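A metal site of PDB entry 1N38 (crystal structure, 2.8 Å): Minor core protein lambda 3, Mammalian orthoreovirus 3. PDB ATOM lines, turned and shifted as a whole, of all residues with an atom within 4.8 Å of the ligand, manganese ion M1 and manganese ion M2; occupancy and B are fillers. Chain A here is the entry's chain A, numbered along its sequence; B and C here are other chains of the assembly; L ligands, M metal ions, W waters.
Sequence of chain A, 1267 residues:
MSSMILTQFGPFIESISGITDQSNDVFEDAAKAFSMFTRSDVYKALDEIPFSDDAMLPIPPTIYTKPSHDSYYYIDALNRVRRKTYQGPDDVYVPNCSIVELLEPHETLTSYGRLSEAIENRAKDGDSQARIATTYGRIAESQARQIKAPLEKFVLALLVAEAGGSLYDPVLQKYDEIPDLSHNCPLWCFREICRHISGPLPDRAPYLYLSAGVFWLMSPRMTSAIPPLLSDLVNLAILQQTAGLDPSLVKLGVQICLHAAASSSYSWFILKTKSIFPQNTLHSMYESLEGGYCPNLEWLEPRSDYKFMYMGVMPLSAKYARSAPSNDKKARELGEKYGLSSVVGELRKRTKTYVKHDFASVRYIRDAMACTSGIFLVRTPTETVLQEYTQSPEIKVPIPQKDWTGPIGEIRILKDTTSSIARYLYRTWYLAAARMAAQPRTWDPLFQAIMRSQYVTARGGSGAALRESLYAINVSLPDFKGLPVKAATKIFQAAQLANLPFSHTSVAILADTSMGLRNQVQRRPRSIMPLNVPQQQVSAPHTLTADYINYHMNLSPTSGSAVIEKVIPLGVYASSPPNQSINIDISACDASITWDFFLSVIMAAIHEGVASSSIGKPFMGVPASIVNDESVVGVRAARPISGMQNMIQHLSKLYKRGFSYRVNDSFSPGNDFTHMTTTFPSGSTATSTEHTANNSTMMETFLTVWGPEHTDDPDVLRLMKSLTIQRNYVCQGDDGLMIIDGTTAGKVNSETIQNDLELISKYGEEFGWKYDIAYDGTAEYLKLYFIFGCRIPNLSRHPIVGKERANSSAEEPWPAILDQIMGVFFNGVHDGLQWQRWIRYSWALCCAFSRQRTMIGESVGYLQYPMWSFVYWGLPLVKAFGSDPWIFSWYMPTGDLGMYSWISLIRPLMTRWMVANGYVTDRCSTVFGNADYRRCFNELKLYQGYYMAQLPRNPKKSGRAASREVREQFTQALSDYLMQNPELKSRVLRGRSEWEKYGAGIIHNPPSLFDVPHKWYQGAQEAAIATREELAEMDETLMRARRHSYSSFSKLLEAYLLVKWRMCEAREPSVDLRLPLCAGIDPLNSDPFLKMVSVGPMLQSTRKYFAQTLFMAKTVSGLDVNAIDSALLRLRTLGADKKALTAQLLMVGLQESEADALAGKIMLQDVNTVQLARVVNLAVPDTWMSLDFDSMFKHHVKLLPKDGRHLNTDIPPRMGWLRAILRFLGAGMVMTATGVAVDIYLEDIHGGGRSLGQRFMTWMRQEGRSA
Ser 587 touches manganese ion M1 (CA to MN, 3.8 Å).
Of the 20 residues printed, 4 come within 4 Å of manganese ion M1.
Manganese ion M2 is bound by an oxygen (O6) of the ligand (2.3 Å) and the side-chain carboxylate (OD1) of Asp 734 (2.3 Å).
Slightly farther from manganese ion M2 lies the side-chain carboxylate (OD2) of Asp 585 (2.8 Å).
Slightly farther from manganese ion M2 lies an oxygen (O5) of the ligand (2.9 Å).
Manganese ion M1 is bound by O10 of the ligand (2.1 Å).
The side-chain carboxylate (OD2) of Asp 734 is bound to manganese ion M1 (2.2 Å).
Manganese ion M1 is bound by O of Ile 586, 2.4 Å away.
Manganese ion M1 is bound by OD1 of Asp 585, at 2.7 Å.
Water W1 lies within hydrogen-bond range of an oxygen (O13) of the ligand (3.1 Å) and the guanidinium group of Arg 524 (3.3 Å).
Water W2 lies within hydrogen-bond range of OE1 of Gln 520 (2.6 Å), OP2 of C 2 of chain C (2.7 Å) and NH1 of Arg 526 (3.3 Å).
NE2 of Gln 520 sits close to NH1 of Arg 523 (3.0 Å).
The backbone NH (N) of Arg 526 sits at hydrogen-bond distance from the backbone carbonyl oxygen (O) of Arg 518, at 2.9 Å.
The side-chain amide nitrogen of Gln 520 lies close to the guanidinium group of Arg 526.
The side-chain carboxylate (OD1) of Asp 590 is in hydrogen-bond range of a ring nitrogen (NE2) of His 691 (2.9 Å).
The side-chain carboxylate of Asp 590 lies within hydrogen-bond range of the side-chain hydroxyl of Ser 682, at 3.4 Å.
N4 of C 2 of chain C lies close to O6 of G 5 of chain B, at 2.6 Å.
O of Thr 687 sits close to ND1 of His 691 (3.5 Å).
OG1 of Thr 687 lies within hydrogen-bond range of O of Ser 682, at 3.1 Å.
CB of Ser 587 touches O12 of the ligand (3.5 Å).
Ala 588 touches the ligand.
CG2 of Thr 687 touches O3 of the ligand, 3.3 Å away.
CD2 of His 691 touches O3 of the ligand, 3.9 Å away.
O2 of C 2 of chain C touches N1 of the ligand (3.6 Å).
Of the 20 residues printed, 14 come within 4 Å of the ligand.
The nearest printed residue that does not touch the ligand is Arg 518 (4.1 Å).
NH2 of Arg 523 is in salt-bridge range of O9 of the ligand, at 2.8 Å.
N1 of A 4 of chain B sits at hydrogen-bond distance from a nitrogen (N2) of the ligand (3.0 Å).
NH2 of Arg 524 lies within salt-bridge range of O9 of the ligand (3.1 Å).
The guanidinium group (NH2) of Arg 526 lies within salt-bridge range of an oxygen (O7) of the ligand, at 3.5 Å.
OD2 of Asp 590 lies within hydrogen-bond range of O3 of the ligand, 3.3 Å away.
A nitrogen (N2) of the ligand lies within hydrogen-bond range of N1 of G 5 of chain B.
Merely in contact with manganese ion M2: Asp 735 (3.1 Å).
Three residues have an atom within 4 Å of manganese ion M2: Asp 585, Asp 734 and Asp 735.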
ATOM      1  N   ARG A 518      -6.117 -31.656  11.131  1.00  0.00           N
ATOM      2  CA  ARG A 518      -4.954 -30.863  11.480  1.00  0.00           C
ATOM      3  C   ARG A 518      -4.781 -30.510  12.951  1.00  0.00           C
ATOM      4  O   ARG A 518      -5.635 -29.851  13.557  1.00  0.00           O
ATOM      5  CB  ARG A 518      -4.951 -29.584  10.662  1.00  0.00           C
ATOM      6  CG  ARG A 518      -3.750 -29.481   9.763  1.00  0.00           C
ATOM      7  CD  ARG A 518      -3.663 -28.122   9.118  1.00  0.00           C
ATOM      8  NE  ARG A 518      -2.269 -27.761   8.910  1.00  0.00           N
ATOM      9  CZ  ARG A 518      -1.435 -28.448   8.140  1.00  0.00           C
ATOM     10  NH1 ARG A 518      -1.867 -29.523   7.495  1.00  0.00           N
ATOM     11  NH2 ARG A 518      -0.178 -28.074   8.033  1.00  0.00           N
ATOM     12  N   GLN A 520      -2.725 -28.603  16.014  1.00  0.00           N
ATOM     13  CA  GLN A 520      -1.992 -27.353  16.209  1.00  0.00           C
ATOM     14  C   GLN A 520      -1.500 -27.273  17.630  1.00  0.00           C
ATOM     15  O   GLN A 520      -2.020 -27.912  18.529  1.00  0.00           O
ATOM     16  CB  GLN A 520      -2.913 -26.161  15.927  1.00  0.00           C
ATOM     17  CG  GLN A 520      -3.647 -26.212  14.581  1.00  0.00           C
ATOM     18  CD  GLN A 520      -4.583 -25.010  14.341  1.00  0.00           C
ATOM     19  OE1 GLN A 520      -4.128 -23.860  14.184  1.00  0.00           O
ATOM     20  NE2 GLN A 520      -5.886 -25.273  14.294  1.00  0.00           N
ATOM     21  N   ARG A 523      -3.924 -25.380  20.504  1.00  0.00           N
ATOM     22  CA  ARG A 523      -5.269 -25.219  19.950  1.00  0.00           C
ATOM     23  C   ARG A 523      -5.930 -26.578  19.710  1.00  0.00           C
ATOM     24  O   ARG A 523      -5.254 -27.598  19.688  1.00  0.00           O
ATOM     25  CB  ARG A 523      -5.234 -24.439  18.614  1.00  0.00           C
ATOM     26  CG  ARG A 523      -6.613 -24.169  18.009  1.00  0.00           C
ATOM     27  CD  ARG A 523      -6.521 -23.462  16.657  1.00  0.00           C
ATOM     28  NE  ARG A 523      -7.832 -23.244  16.035  1.00  0.00           N
ATOM     29  CZ  ARG A 523      -8.695 -24.215  15.714  1.00  0.00           C
ATOM     30  NH1 ARG A 523      -8.395 -25.472  15.957  1.00  0.00           N
ATOM     31  NH2 ARG A 523      -9.857 -23.919  15.144  1.00  0.00           N
ATOM     32  N   ARG A 524      -7.252 -26.601  19.542  1.00  0.00           N
ATOM     33  CA  ARG A 524      -7.940 -27.857  19.309  1.00  0.00           C
ATOM     34  C   ARG A 524      -7.708 -28.304  17.865  1.00  0.00           C
ATOM     35  O   ARG A 524      -7.348 -27.486  17.019  1.00  0.00           O
ATOM     36  CB  ARG A 524      -9.447 -27.709  19.555  1.00  0.00           C
ATOM     37  CG  ARG A 524     -10.131 -26.713  18.627  1.00  0.00           C
ATOM     38  CD  ARG A 524     -11.590 -26.502  19.015  1.00  0.00           C
ATOM     39  NE  ARG A 524     -12.285 -25.592  18.098  1.00  0.00           N
ATOM     40  CZ  ARG A 524     -11.919 -24.342  17.857  1.00  0.00           C
ATOM     41  NH1 ARG A 524     -10.852 -23.807  18.454  1.00  0.00           N
ATOM     42  NH2 ARG A 524     -12.618 -23.591  17.024  1.00  0.00           N
ATOM     43  N   ARG A 526      -8.426 -29.215  14.081  1.00  0.00           N
ATOM     44  CA  ARG A 526      -9.424 -28.709  13.165  1.00  0.00           C
ATOM     45  C   ARG A 526      -9.648 -29.647  11.979  1.00  0.00           C
ATOM     46  O   ARG A 526      -8.713 -30.210  11.426  1.00  0.00           O
ATOM     47  CB  ARG A 526      -9.038 -27.315  12.654  1.00  0.00           C
ATOM     48  CG  ARG A 526      -7.879 -27.288  11.676  1.00  0.00           C
ATOM     49  CD  ARG A 526      -8.057 -26.173  10.661  1.00  0.00           C
ATOM     50  NE  ARG A 526      -8.135 -24.857  11.286  1.00  0.00           N
ATOM     51  CZ  ARG A 526      -7.080 -24.194  11.762  1.00  0.00           C
ATOM     52  NH1 ARG A 526      -5.864 -24.717  11.682  1.00  0.00           N
ATOM     53  NH2 ARG A 526      -7.252 -23.006  12.319  1.00  0.00           N
ATOM     54  N   ASP A 585     -11.012 -10.558  16.696  1.00  0.00           N
ATOM     55  CA  ASP A 585     -11.008 -11.920  16.206  1.00  0.00           C
ATOM     56  C   ASP A 585     -12.470 -12.330  16.212  1.00  0.00           C
ATOM     57  O   ASP A 585     -13.283 -11.747  16.931  1.00  0.00           O
ATOM     58  CB  ASP A 585     -10.148 -12.790  17.147  1.00  0.00           C
ATOM     59  CG  ASP A 585      -9.948 -14.214  16.629  1.00  0.00           C
ATOM     60  OD1 ASP A 585     -10.789 -15.084  16.945  1.00  0.00           O
ATOM     61  OD2 ASP A 585      -8.958 -14.462  15.895  1.00  0.00           O
ATOM     62  N   ILE A 586     -12.832 -13.306  15.382  1.00  0.00           N
ATOM     63  CA  ILE A 586     -14.204 -13.787  15.310  1.00  0.00           C
ATOM     64  C   ILE A 586     -14.169 -15.274  15.584  1.00  0.00           C
ATOM     65  O   ILE A 586     -13.579 -16.036  14.818  1.00  0.00           O
ATOM     66  CB  ILE A 586     -14.794 -13.520  13.917  1.00  0.00           C
ATOM     67  CG1 ILE A 586     -14.723 -12.026  13.602  1.00  0.00           C
ATOM     68  CG2 ILE A 586     -16.235 -13.954  13.853  1.00  0.00           C
ATOM     69  CD1 ILE A 586     -14.897 -11.721  12.143  1.00  0.00           C
ATOM     70  N   SER A 587     -14.778 -15.698  16.691  1.00  0.00           N
ATOM     71  CA  SER A 587     -14.756 -17.118  17.011  1.00  0.00           C
ATOM     72  C   SER A 587     -15.763 -17.947  16.229  1.00  0.00           C
ATOM     73  O   SER A 587     -16.917 -17.545  16.023  1.00  0.00           O
ATOM     74  CB  SER A 587     -14.915 -17.329  18.525  1.00  0.00           C
ATOM     75  OG  SER A 587     -16.022 -16.624  19.040  1.00  0.00           O
ATOM     76  N   ALA A 588     -15.294 -19.109  15.788  1.00  0.00           N
ATOM     77  CA  ALA A 588     -16.100 -20.037  15.018  1.00  0.00           C
ATOM     78  C   ALA A 588     -16.425 -19.427  13.661  1.00  0.00           C
ATOM     79  O   ALA A 588     -17.521 -19.603  13.155  1.00  0.00           O
ATOM     80  CB  ALA A 588     -17.388 -20.359  15.758  1.00  0.00           C
ATOM     81  N   CYS A 589     -15.470 -18.711  13.080  1.00  0.00           N
ATOM     82  CA  CYS A 589     -15.693 -18.058  11.800  1.00  0.00           C
ATOM     83  C   CYS A 589     -16.369 -18.974  10.779  1.00  0.00           C
ATOM     84  O   CYS A 589     -17.442 -18.636  10.266  1.00  0.00           O
ATOM     85  CB  CYS A 589     -14.378 -17.511  11.234  1.00  0.00           C
ATOM     86  SG  CYS A 589     -14.625 -16.475   9.760  1.00  0.00           S
ATOM     87  N   ASP A 590     -15.740 -20.121  10.489  1.00  0.00           N
ATOM     88  CA  ASP A 590     -16.281 -21.067   9.510  1.00  0.00           C
ATOM     89  C   ASP A 590     -17.731 -21.471   9.771  1.00  0.00           C
ATOM     90  O   ASP A 590     -18.526 -21.564   8.830  1.00  0.00           O
ATOM     91  CB  ASP A 590     -15.389 -22.321   9.409  1.00  0.00           C
ATOM     92  CG  ASP A 590     -14.121 -22.062   8.613  1.00  0.00           C
ATOM     93  OD1 ASP A 590     -14.211 -21.369   7.577  1.00  0.00           O
ATOM     94  OD2 ASP A 590     -13.027 -22.546   8.994  1.00  0.00           O
ATOM     95  N   SER A 682     -12.926 -25.270   4.569  1.00  0.00           N
ATOM     96  CA  SER A 682     -11.589 -24.716   4.744  1.00  0.00           C
ATOM     97  C   SER A 682     -10.766 -25.002   3.485  1.00  0.00           C
ATOM     98  O   SER A 682      -9.942 -24.186   3.042  1.00  0.00           O
ATOM     99  CB  SER A 682     -10.918 -25.336   5.968  1.00  0.00           C
ATOM    100  OG  SER A 682     -11.597 -24.988   7.163  1.00  0.00           O
ATOM    101  N   THR A 687     -12.419 -19.697   0.903  1.00  0.00           N
ATOM    102  CA  THR A 687     -12.254 -19.608   2.364  1.00  0.00           C
ATOM    103  C   THR A 687     -11.547 -18.367   2.919  1.00  0.00           C
ATOM    104  O   THR A 687     -12.190 -17.424   3.384  1.00  0.00           O
ATOM    105  CB  THR A 687     -11.513 -20.851   2.913  1.00  0.00           C
ATOM    106  OG1 THR A 687     -12.079 -22.047   2.349  1.00  0.00           O
ATOM    107  CG2 THR A 687     -11.629 -20.916   4.424  1.00  0.00           C
ATOM    108  N   HIS A 691     -13.442 -14.814   3.946  1.00  0.00           N
ATOM    109  CA  HIS A 691     -13.592 -14.329   5.304  1.00  0.00           C
ATOM    110  C   HIS A 691     -12.919 -12.979   5.479  1.00  0.00           C
ATOM    111  O   HIS A 691     -13.432 -12.117   6.194  1.00  0.00           O
ATOM    112  CB  HIS A 691     -13.024 -15.361   6.279  1.00  0.00           C
ATOM    113  CG  HIS A 691     -13.722 -16.677   6.215  1.00  0.00           C
ATOM    114  ND1 HIS A 691     -14.895 -16.880   5.507  1.00  0.00           N
ATOM    115  CD2 HIS A 691     -13.413 -17.878   6.767  1.00  0.00           C
ATOM    116  CE1 HIS A 691     -15.276 -18.135   5.628  1.00  0.00           C
ATOM    117  NE2 HIS A 691     -14.400 -18.766   6.398  1.00  0.00           N
ATOM    118  N   ASP A 734     -10.225 -14.157   9.714  1.00  0.00           N
ATOM    119  CA  ASP A 734     -11.085 -13.734  10.805  1.00  0.00           C
ATOM    120  C   ASP A 734     -10.290 -12.941  11.839  1.00  0.00           C
ATOM    121  O   ASP A 734     -10.770 -12.706  12.952  1.00  0.00           O
ATOM    122  CB  ASP A 734     -11.743 -14.945  11.451  1.00  0.00           C
ATOM    123  CG  ASP A 734     -10.761 -15.815  12.228  1.00  0.00           C
ATOM    124  OD1 ASP A 734      -9.527 -15.705  12.001  1.00  0.00           O
ATOM    125  OD2 ASP A 734     -11.232 -16.616  13.069  1.00  0.00           O
ATOM    126  N   ASP A 735      -9.084 -12.519  11.477  1.00  0.00           N
ATOM    127  CA  ASP A 735      -8.274 -11.742  12.393  1.00  0.00           C
ATOM    128  C   ASP A 735      -8.298 -10.269  12.045  1.00  0.00           C
ATOM    129  O   ASP A 735      -8.180  -9.887  10.892  1.00  0.00           O
ATOM    130  CB  ASP A 735      -6.822 -12.225  12.418  1.00  0.00           C
ATOM    131  CG  ASP A 735      -6.365 -12.587  13.811  1.00  0.00           C
ATOM    132  OD1 ASP A 735      -6.752 -13.687  14.260  1.00  0.00           O
ATOM    133  OD2 ASP A 735      -5.676 -11.765  14.471  1.00  0.00           O
ATOM    134  N   LYS A 783      -0.901 -14.208  15.125  1.00  0.00           N
ATOM    135  CA  LYS A 783      -0.069 -14.893  16.122  1.00  0.00           C
ATOM    136  C   LYS A 783       1.289 -14.227  16.361  1.00  0.00           C
ATOM    137  O   LYS A 783       2.274 -14.883  16.721  1.00  0.00           O
ATOM    138  CB  LYS A 783       0.107 -16.369  15.747  1.00  0.00           C
ATOM    139  CG  LYS A 783      -1.182 -17.204  15.856  1.00  0.00           C
ATOM    140  CD  LYS A 783      -1.611 -17.369  17.304  1.00  0.00           C
ATOM    141  CE  LYS A 783      -2.916 -18.149  17.433  1.00  0.00           C
ATOM    142  NZ  LYS A 783      -4.098 -17.404  16.930  1.00  0.00           N
ATOM    143  P     A B   4      -4.213 -33.010   1.796  1.00  0.00           P
ATOM    144  OP1   A B   4      -4.012 -33.994   0.711  1.00  0.00           O
ATOM    145  OP2   A B   4      -3.048 -32.508   2.543  1.00  0.00           O
ATOM    146  O5'   A B   4      -4.983 -31.759   1.178  1.00  0.00           O
ATOM    147  C5'   A B   4      -6.076 -31.947   0.294  1.00  0.00           C
ATOM    148  C4'   A B   4      -6.974 -30.735   0.270  1.00  0.00           C
ATOM    149  O4'   A B   4      -7.540 -30.513   1.582  1.00  0.00           O
ATOM    150  C3'   A B   4      -6.305 -29.418  -0.060  1.00  0.00           C
ATOM    151  O3'   A B   4      -6.152 -29.250  -1.459  1.00  0.00           O
ATOM    152  C2'   A B   4      -7.296 -28.425   0.507  1.00  0.00           C
ATOM    153  O2'   A B   4      -8.445 -28.325  -0.315  1.00  0.00           O
ATOM    154  C1'   A B   4      -7.676 -29.120   1.813  1.00  0.00           C
ATOM    155  N9    A B   4      -6.802 -28.758   2.922  1.00  0.00           N
ATOM    156  C8    A B   4      -5.833 -29.536   3.506  1.00  0.00           C
ATOM    157  N7    A B   4      -5.237 -28.954   4.518  1.00  0.00           N
ATOM    158  C5    A B   4      -5.830 -27.703   4.590  1.00  0.00           C
ATOM    159  C6    A B   4      -5.642 -26.611   5.463  1.00  0.00           C
ATOM    160  N6    A B   4      -4.762 -26.613   6.453  1.00  0.00           N
ATOM    161  N1    A B   4      -6.404 -25.516   5.266  1.00  0.00           N
ATOM    162  C2    A B   4      -7.294 -25.518   4.268  1.00  0.00           C
ATOM    163  N3    A B   4      -7.561 -26.484   3.386  1.00  0.00           N
ATOM    164  C4    A B   4      -6.796 -27.565   3.610  1.00  0.00           C
ATOM    165  P     G B   5      -5.135 -28.150  -2.019  1.00  0.00           P
ATOM    166  OP1   G B   5      -5.188 -28.184  -3.491  1.00  0.00           O
ATOM    167  OP2   G B   5      -3.857 -28.407  -1.338  1.00  0.00           O
ATOM    168  O5'   G B   5      -5.720 -26.756  -1.512  1.00  0.00           O
ATOM    169  C5'   G B   5      -6.816 -26.141  -2.186  1.00  0.00           C
ATOM    170  C4'   G B   5      -6.967 -24.697  -1.765  1.00  0.00           C
ATOM    171  O4'   G B   5      -7.314 -24.623  -0.361  1.00  0.00           O
ATOM    172  C3'   G B   5      -5.719 -23.826  -1.888  1.00  0.00           C
ATOM    173  O3'   G B   5      -5.628 -23.306  -3.210  1.00  0.00           O
ATOM    174  C2'   G B   5      -5.999 -22.711  -0.893  1.00  0.00           C
ATOM    175  O2'   G B   5      -6.810 -21.663  -1.400  1.00  0.00           O
ATOM    176  C1'   G B   5      -6.727 -23.472   0.223  1.00  0.00           C
ATOM    177  N9    G B   5      -5.794 -23.913   1.250  1.00  0.00           N
ATOM    178  C8    G B   5      -5.115 -25.106   1.284  1.00  0.00           C
ATOM    179  N7    G B   5      -4.361 -25.234   2.344  1.00  0.00           N
ATOM    180  C5    G B   5      -4.546 -24.045   3.038  1.00  0.00           C
ATOM    181  C6    G B   5      -3.989 -23.606   4.254  1.00  0.00           C
ATOM    182  O6    G B   5      -3.188 -24.204   4.983  1.00  0.00           O
ATOM    183  N1    G B   5      -4.435 -22.329   4.610  1.00  0.00           N
ATOM    184  C2    G B   5      -5.324 -21.582   3.872  1.00  0.00           C
ATOM    185  N2    G B   5      -5.661 -20.355   4.386  1.00  0.00           N
ATOM    186  N3    G B   5      -5.862 -21.989   2.717  1.00  0.00           N
ATOM    187  C4    G B   5      -5.424 -23.216   2.370  1.00  0.00           C
ATOM    188  P     C C   2      -0.847 -20.238  12.964  1.00  0.00           P
ATOM    189  OP1   C C   2      -1.352 -20.555  14.319  1.00  0.00           O
ATOM    190  OP2   C C   2      -1.133 -21.161  11.836  1.00  0.00           O
ATOM    191  O5'   C C   2      -1.421 -18.792  12.582  1.00  0.00           O
ATOM    192  C5'   C C   2      -2.813 -18.527  12.763  1.00  0.00           C
ATOM    193  C4'   C C   2      -3.387 -17.802  11.562  1.00  0.00           C
ATOM    194  O4'   C C   2      -2.550 -17.975  10.391  1.00  0.00           O
ATOM    195  C3'   C C   2      -4.753 -18.331  11.151  1.00  0.00           C
ATOM    196  C2'   C C   2      -4.828 -17.989   9.670  1.00  0.00           C
ATOM    197  O2'   C C   2      -5.323 -16.677   9.460  1.00  0.00           O
ATOM    198  C1'   C C   2      -3.363 -18.080   9.231  1.00  0.00           C
ATOM    199  N1    C C   2      -2.926 -19.276   8.461  1.00  0.00           N
ATOM    200  C2    C C   2      -3.727 -19.792   7.398  1.00  0.00           C
ATOM    201  O2    C C   2      -4.834 -19.266   7.144  1.00  0.00           O
ATOM    202  N3    C C   2      -3.261 -20.841   6.673  1.00  0.00           N
ATOM    203  C4    C C   2      -2.090 -21.399   6.968  1.00  0.00           C
ATOM    204  N4    C C   2      -1.677 -22.411   6.208  1.00  0.00           N
ATOM    205  C5    C C   2      -1.277 -20.919   8.048  1.00  0.00           C
ATOM    206  C6    C C   2      -1.725 -19.875   8.762  1.00  0.00           C
HETATM  207  N1  LIG L   1      -7.377 -21.324   8.534  1.00  0.00           N
HETATM  208  C1  LIG L   1      -6.337 -21.582   9.407  1.00  0.00           C
HETATM  209  C2  LIG L   1      -7.269 -22.335   7.272  1.00  0.00           C
HETATM  210  O1  LIG L   1      -8.088 -22.293   6.355  1.00  0.00           O
HETATM  211  N2  LIG L   1      -6.224 -23.251   7.270  1.00  0.00           N
HETATM  212  C3  LIG L   1      -5.231 -23.395   8.238  1.00  0.00           C
HETATM  213  O2  LIG L   1      -4.364 -24.255   8.096  1.00  0.00           O
HETATM  214  C4  LIG L   1      -5.337 -22.484   9.371  1.00  0.00           C
HETATM  215  C5  LIG L   1      -8.532 -20.320   8.517  1.00  0.00           C
HETATM  216  C6  LIG L   1      -9.943 -20.909   8.721  1.00  0.00           C
HETATM  217  O3  LIG L   1     -10.767 -20.556   7.622  1.00  0.00           O
HETATM  218  C7  LIG L   1     -10.451 -20.411  10.042  1.00  0.00           C
HETATM  219  C8  LIG L   1      -9.576 -19.217  10.337  1.00  0.00           C
HETATM  220  O4  LIG L   1      -8.413 -19.229   9.480  1.00  0.00           O
HETATM  221  C9  LIG L   1      -9.490 -19.018  11.866  1.00  0.00           C
HETATM  222  O5  LIG L   1      -8.221 -18.864  12.473  1.00  0.00           O
HETATM  223  P1  LIG L   1      -8.014 -19.451  14.016  1.00  0.00           P
HETATM  224  O6  LIG L   1      -8.208 -18.285  15.040  1.00  0.00           O
HETATM  225  O7  LIG L   1      -6.579 -20.037  14.085  1.00  0.00           O
HETATM  226  O8  LIG L   1      -9.265 -20.596  14.087  1.00  0.00           O
HETATM  227  P2  LIG L   1     -10.542 -20.466  15.138  1.00  0.00           P
HETATM  228  O9  LIG L   1     -11.478 -21.703  14.851  1.00  0.00           O
HETATM  229  O10 LIG L   1     -11.345 -19.143  14.885  1.00  0.00           O
HETATM  230  O11 LIG L   1      -9.950 -20.683  16.697  1.00  0.00           O
HETATM  231  P3  LIG L   1     -10.766 -20.230  18.062  1.00  0.00           P
HETATM  232  O12 LIG L   1     -12.106 -19.427  18.060  1.00  0.00           O
HETATM  233  O13 LIG L   1      -9.999 -20.538  19.429  1.00  0.00           O
HETATM  234  O14 LIG L   1     -10.022 -18.841  17.912  1.00  0.00           O
HETATM  235 MN    MN M   1     -11.391 -17.022  15.193  1.00  0.00          MN
HETATM  236 MN    MN M   2      -8.371 -16.330  13.885  1.00  0.00          MN
HETATM  237  O   HOH W   1      -8.259 -22.969  20.395  1.00  0.00           O
HETATM  238  O   HOH W   2      -3.452 -22.464  12.114  1.00  0.00           O
HETATM  239  O   HOH W   3      -9.280 -17.900   6.445  1.00  0.00           O
HETATM  240  O   HOH W   4     -13.182 -22.192  12.607  1.00  0.00           O
